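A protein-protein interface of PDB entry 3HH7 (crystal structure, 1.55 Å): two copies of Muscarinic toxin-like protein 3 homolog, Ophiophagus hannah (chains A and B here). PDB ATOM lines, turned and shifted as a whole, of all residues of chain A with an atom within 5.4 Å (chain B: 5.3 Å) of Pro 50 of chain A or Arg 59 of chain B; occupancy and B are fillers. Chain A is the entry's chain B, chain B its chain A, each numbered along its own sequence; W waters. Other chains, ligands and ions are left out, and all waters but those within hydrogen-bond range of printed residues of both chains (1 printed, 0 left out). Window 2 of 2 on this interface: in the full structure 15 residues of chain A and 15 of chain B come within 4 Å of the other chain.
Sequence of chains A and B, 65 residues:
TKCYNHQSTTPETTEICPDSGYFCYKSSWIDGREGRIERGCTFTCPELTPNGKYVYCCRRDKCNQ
The guanidinium group of Arg 59 of chain B lies within hydrogen-bond range of the backbone carbonyl oxygen of Thr 49 of chain A, at 2.7 Å.
The guanidinium group (NH2) of Arg 59 of chain B sits close to the backbone carbonyl oxygen (O) of Pro 50 of chain A (3.3 Å).
NE of Arg 59 of chain B sits at hydrogen-bond distance from O of Gly 52 of chain A, at 2.8 Å.
The backbone NH of Arg 59 of chain B lies within hydrogen-bond range of the backbone carbonyl oxygen of Lys 53 of chain A (3.4 Å).
The backbone NH of Cys 24 of chain B sits at hydrogen-bond distance from the backbone carbonyl oxygen of Cys 58 of chain B, at 2.8 Å.
SG of Cys 58 of chain B is disulfide-bonded to SG of Cys 63 of chain B.
The backbone NH (N) of Arg 59 of chain B lies within hydrogen-bond range of the side-chain sulfur (SG) of Cys 63 of chain B, 3.7 Å away.
The side-chain hydroxyl of Thr 49 of chain A lies within hydrogen-bond range of the backbone NH of Gly 52 of chain A (3.2 Å).
Among the printed residues, merely in contact across the chains: Leu 48 of chain A with Phe 23 of chain B (3.6 Å) and Lys 53 of chain A with Cys 58 of chain B (3.6 Å).
Printed residues of chain B within 4 Å of Leu 48 of chain A: Phe 23 (3.6 Å).
Of chain B, only Arg 59 (3.3 Å) comes within 4 Å of Pro 50 of chain A.
Of the printed residues of chain B, Gly 52 of chain A touches Arg 59.
Of the printed residues of chain B, Lys 53 of chain A touches Cys 58 and Arg 59.
Printed residues of chain A within 4 Å of Cys 58 of chain B: Lys 53 (3.6 Å).
Arg 59 of chain B touches four residues of chain A.
Of the 11 printed residues of chain B, 3 touch a printed residue of chain A.
Printed residues of chain B that touch a printed residue of chain A: Phe 23, Cys 58 and Arg 59.
Hydrophobic or aromatic side chains of chain B that line the printed part of chain A: Phe 23.
Of the 6 printed residues of chain A, 5 touch a printed residue of chain B.
Printed residues of chain A that touch a printed residue of chain B: Leu 48, Thr 49, Pro 50, Gly 52 and Lys 53.
Among the printed residues, 6 pairs touch across the chains.
Among the printed residues, no Asp or Glu carboxylate lies within 4 Å of a Lys or Arg side-chain nitrogen of the other chain.
No position is printed for both chains.
Of the 6 pairs that touch across the chains among the printed residues, none has its exchanged pair printed and touching as well.
Water W1 lies within hydrogen-bond range of the backbone carbonyl oxygen of Lys 53 of chain A and the backbone NH of Arg 59 of chain B.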
ATOM      1  N   LEU A  48     -23.327 -11.805  -6.453  1.00  0.00           N
ATOM      2  CA  LEU A  48     -23.273 -12.759  -7.566  1.00  0.00           C
ATOM      3  C   LEU A  48     -23.858 -12.045  -8.780  1.00  0.00           C
ATOM      4  O   LEU A  48     -25.057 -11.749  -8.804  1.00  0.00           O
ATOM      5  CB  LEU A  48     -24.033 -14.057  -7.242  1.00  0.00           C
ATOM      6  CG  LEU A  48     -23.940 -15.134  -8.344  1.00  0.00           C
ATOM      7  CD1 LEU A  48     -22.529 -15.589  -8.536  1.00  0.00           C
ATOM      8  CD2 LEU A  48     -24.826 -16.335  -8.048  1.00  0.00           C
ATOM      9  N   THR A  49     -22.973 -11.735  -9.735  1.00  0.00           N
ATOM     10  CA  THR A  49     -23.312 -11.011 -10.969  1.00  0.00           C
ATOM     11  C   THR A  49     -24.089 -11.908 -11.918  1.00  0.00           C
ATOM     12  O   THR A  49     -24.059 -13.124 -11.773  1.00  0.00           O
ATOM     13  CB  THR A  49     -22.039 -10.535 -11.706  1.00  0.00           C
ATOM     14  OG1 THR A  49     -21.232 -11.678 -12.065  1.00  0.00           O
ATOM     15  CG2 THR A  49     -21.228  -9.611 -10.837  1.00  0.00           C
ATOM     16  N   PRO A  50     -24.812 -11.310 -12.892  1.00  0.00           N
ATOM     17  CA  PRO A  50     -25.568 -12.153 -13.836  1.00  0.00           C
ATOM     18  C   PRO A  50     -24.781 -13.284 -14.510  1.00  0.00           C
ATOM     19  O   PRO A  50     -25.326 -14.374 -14.694  1.00  0.00           O
ATOM     20  CB  PRO A  50     -26.085 -11.141 -14.860  1.00  0.00           C
ATOM     21  CG  PRO A  50     -26.289  -9.895 -14.022  1.00  0.00           C
ATOM     22  CD  PRO A  50     -25.063  -9.878 -13.130  1.00  0.00           C
ATOM     23  N   ASN A  51     -23.514 -13.049 -14.833  1.00  0.00           N
ATOM     24  CA  ASN A  51     -22.714 -14.095 -15.470  1.00  0.00           C
ATOM     25  C   ASN A  51     -21.840 -14.877 -14.463  1.00  0.00           C
ATOM     26  O   ASN A  51     -21.058 -15.767 -14.827  1.00  0.00           O
ATOM     27  CB  ASN A  51     -21.936 -13.507 -16.654  1.00  0.00           C
ATOM     28  CG  ASN A  51     -22.749 -12.439 -17.416  1.00  0.00           C
ATOM     29  OD1 ASN A  51     -23.614 -12.751 -18.253  1.00  0.00           O
ATOM     30  ND2 ASN A  51     -22.485 -11.161 -17.103  1.00  0.00           N
ATOM     31  N   GLY A  52     -22.001 -14.554 -13.181  1.00  0.00           N
ATOM     32  CA  GLY A  52     -21.366 -15.331 -12.120  1.00  0.00           C
ATOM     33  C   GLY A  52     -21.974 -16.721 -12.023  1.00  0.00           C
ATOM     34  O   GLY A  52     -23.185 -16.895 -12.226  1.00  0.00           O
ATOM     35  N   LYS A  53     -21.140 -17.722 -11.764  1.00  0.00           N
ATOM     36  CA  LYS A  53     -21.575 -19.094 -11.531  1.00  0.00           C
ATOM     37  C   LYS A  53     -21.808 -19.325 -10.034  1.00  0.00           C
ATOM     38  O   LYS A  53     -22.810 -19.916  -9.616  1.00  0.00           O
ATOM     39  CB  LYS A  53     -20.527 -20.087 -12.050  1.00  0.00           C
ATOM     40  CG  LYS A  53     -20.424 -20.116 -13.572  1.00  0.00           C
ATOM     41  CD  LYS A  53     -19.620 -21.315 -14.048  1.00  0.00           C
ATOM     42  CE  LYS A  53     -18.143 -20.980 -14.175  1.00  0.00           C
ATOM     43  NZ  LYS A  53     -17.359 -22.145 -14.716  1.00  0.00           N
ATOM     44  N   THR B   1     -35.206 -21.816 -11.917  1.00  0.00           N
ATOM     45  CA  THR B   1     -34.313 -22.107 -10.750  1.00  0.00           C
ATOM     46  C   THR B   1     -35.075 -22.805  -9.628  1.00  0.00           C
ATOM     47  O   THR B   1     -36.107 -22.320  -9.180  1.00  0.00           O
ATOM     48  CB  THR B   1     -33.683 -20.807 -10.206  1.00  0.00           C
ATOM     49  OG1 THR B   1     -33.128 -20.059 -11.291  1.00  0.00           O
ATOM     50  CG2 THR B   1     -32.588 -21.120  -9.213  1.00  0.00           C
ATOM     51  N   SER B  20     -36.431 -14.485 -12.956  1.00  0.00           N
ATOM     52  CA  SER B  20     -35.217 -14.941 -13.634  1.00  0.00           C
ATOM     53  C   SER B  20     -33.930 -14.483 -12.949  1.00  0.00           C
ATOM     54  O   SER B  20     -32.885 -15.141 -13.058  1.00  0.00           O
ATOM     55  CB  SER B  20     -35.227 -14.557 -15.123  1.00  0.00           C
ATOM     56  OG  SER B  20     -36.052 -13.430 -15.385  1.00  0.00           O
ATOM     57  N   TYR B  22     -33.010 -14.796 -10.103  1.00  0.00           N
ATOM     58  CA  TYR B  22     -32.882 -15.578  -8.874  1.00  0.00           C
ATOM     59  C   TYR B  22     -31.894 -16.711  -8.963  1.00  0.00           C
ATOM     60  O   TYR B  22     -31.790 -17.416  -9.966  1.00  0.00           O
ATOM     61  CB  TYR B  22     -34.229 -16.159  -8.452  1.00  0.00           C
ATOM     62  CG  TYR B  22     -35.121 -15.172  -7.766  1.00  0.00           C
ATOM     63  CD1 TYR B  22     -35.220 -15.139  -6.376  1.00  0.00           C
ATOM     64  CD2 TYR B  22     -35.867 -14.257  -8.504  1.00  0.00           C
ATOM     65  CE1 TYR B  22     -36.039 -14.228  -5.740  1.00  0.00           C
ATOM     66  CE2 TYR B  22     -36.691 -13.339  -7.877  1.00  0.00           C
ATOM     67  CZ  TYR B  22     -36.776 -13.329  -6.501  1.00  0.00           C
ATOM     68  OH  TYR B  22     -37.594 -12.419  -5.891  1.00  0.00           O
ATOM     69  N   PHE B  23     -31.187 -16.896  -7.860  1.00  0.00           N
ATOM     70  CA  PHE B  23     -30.266 -18.005  -7.694  1.00  0.00           C
ATOM     71  C   PHE B  23     -30.452 -18.570  -6.292  1.00  0.00           C
ATOM     72  O   PHE B  23     -31.363 -18.148  -5.564  1.00  0.00           O
ATOM     73  CB  PHE B  23     -28.827 -17.548  -7.953  1.00  0.00           C
ATOM     74  CG  PHE B  23     -28.459 -16.238  -7.281  1.00  0.00           C
ATOM     75  CD1 PHE B  23     -28.675 -15.019  -7.927  1.00  0.00           C
ATOM     76  CD2 PHE B  23     -27.849 -16.229  -6.029  1.00  0.00           C
ATOM     77  CE1 PHE B  23     -28.307 -13.822  -7.335  1.00  0.00           C
ATOM     78  CE2 PHE B  23     -27.487 -15.025  -5.430  1.00  0.00           C
ATOM     79  CZ  PHE B  23     -27.717 -13.820  -6.084  1.00  0.00           C
ATOM     80  N   CYS B  24     -29.622 -19.536  -5.930  1.00  0.00           N
ATOM     81  CA  CYS B  24     -29.737 -20.193  -4.626  1.00  0.00           C
ATOM     82  C   CYS B  24     -28.672 -19.716  -3.659  1.00  0.00           C
ATOM     83  O   CYS B  24     -27.568 -19.299  -4.064  1.00  0.00           O
ATOM     84  CB  CYS B  24     -29.587 -21.706  -4.779  1.00  0.00           C
ATOM     85  SG  CYS B  24     -30.666 -22.450  -6.016  1.00  0.00           S
ATOM     86  N   CYS B  57     -23.403 -18.918  -2.776  1.00  0.00           N
ATOM     87  CA  CYS B  57     -24.428 -18.493  -3.725  1.00  0.00           C
ATOM     88  C   CYS B  57     -24.125 -19.148  -5.053  1.00  0.00           C
ATOM     89  O   CYS B  57     -23.003 -19.075  -5.522  1.00  0.00           O
ATOM     90  CB  CYS B  57     -24.456 -16.961  -3.876  1.00  0.00           C
ATOM     91  SG  CYS B  57     -24.925 -16.159  -2.337  1.00  0.00           S
ATOM     92  N   CYS B  58     -25.125 -19.794  -5.640  1.00  0.00           N
ATOM     93  CA  CYS B  58     -24.904 -20.630  -6.805  1.00  0.00           C
ATOM     94  C   CYS B  58     -26.159 -20.671  -7.668  1.00  0.00           C
ATOM     95  O   CYS B  58     -27.273 -20.426  -7.182  1.00  0.00           O
ATOM     96  CB  CYS B  58     -24.463 -22.023  -6.350  1.00  0.00           C
ATOM     97  SG  CYS B  58     -25.654 -22.864  -5.282  1.00  0.00           S
ATOM     98  N   ARG B  59     -25.971 -20.970  -8.957  1.00  0.00           N
ATOM     99  CA  ARG B  59     -27.065 -20.886  -9.930  1.00  0.00           C
ATOM    100  C   ARG B  59     -27.746 -22.203 -10.326  1.00  0.00           C
ATOM    101  O   ARG B  59     -28.915 -22.190 -10.698  1.00  0.00           O
ATOM    102  CB  ARG B  59     -26.595 -20.174 -11.204  1.00  0.00           C
ATOM    103  CG  ARG B  59     -26.260 -18.731 -10.991  1.00  0.00           C
ATOM    104  CD  ARG B  59     -26.261 -17.990 -12.300  1.00  0.00           C
ATOM    105  NE  ARG B  59     -25.918 -16.596 -12.065  1.00  0.00           N
ATOM    106  CZ  ARG B  59     -26.793 -15.654 -11.732  1.00  0.00           C
ATOM    107  NH1 ARG B  59     -28.082 -15.941 -11.602  1.00  0.00           N
ATOM    108  NH2 ARG B  59     -26.370 -14.410 -11.525  1.00  0.00           N
ATOM    109  N   ARG B  60     -27.035 -23.320 -10.259  1.00  0.00           N
ATOM    110  CA  ARG B  60     -27.605 -24.564 -10.796  1.00  0.00           C
ATOM    111  C   ARG B  60     -28.706 -25.103  -9.874  1.00  0.00           C
ATOM    112  O   ARG B  60     -28.664 -24.898  -8.660  1.00  0.00           O
ATOM    113  CB  ARG B  60     -26.507 -25.600 -11.017  1.00  0.00           C
ATOM    114  CG  ARG B  60     -25.408 -25.129 -11.980  1.00  0.00           C
ATOM    115  CD  ARG B  60     -25.889 -24.976 -13.430  1.00  0.00           C
ATOM    116  NE  ARG B  60     -26.360 -26.250 -13.965  1.00  0.00           N
ATOM    117  CZ  ARG B  60     -25.555 -27.185 -14.467  1.00  0.00           C
ATOM    118  NH1 ARG B  60     -24.240 -26.991 -14.510  1.00  0.00           N
ATOM    119  NH2 ARG B  60     -26.067 -28.331 -14.900  1.00  0.00           N
ATOM    120  N   ASP B  61     -29.706 -25.772 -10.447  1.00  0.00           N
ATOM    121  CA  ASP B  61     -30.755 -26.372  -9.637  1.00  0.00           C
ATOM    122  C   ASP B  61     -30.170 -27.293  -8.578  1.00  0.00           C
ATOM    123  O   ASP B  61     -29.292 -28.103  -8.875  1.00  0.00           O
ATOM    124  CB  ASP B  61     -31.728 -27.157 -10.514  1.00  0.00           C
ATOM    125  CG  ASP B  61     -32.770 -26.272 -11.166  1.00  0.00           C
ATOM    126  OD1 ASP B  61     -32.620 -25.031 -11.146  1.00  0.00           O
ATOM    127  OD2 ASP B  61     -33.727 -26.840 -11.714  1.00  0.00           O
ATOM    128  N   CYS B  63     -28.137 -26.673  -6.258  1.00  0.00           N
ATOM    129  CA  CYS B  63     -26.706 -26.471  -6.055  1.00  0.00           C
ATOM    130  C   CYS B  63     -26.337 -26.179  -4.592  1.00  0.00           C
ATOM    131  O   CYS B  63     -25.158 -26.262  -4.196  1.00  0.00           O
ATOM    132  CB  CYS B  63     -26.190 -25.346  -6.963  1.00  0.00           C
ATOM    133  SG  CYS B  63     -26.921 -23.705  -6.644  1.00  0.00           S
HETATM  134  O   HOH W   1     -23.713 -21.723 -10.927  1.00  0.00           O
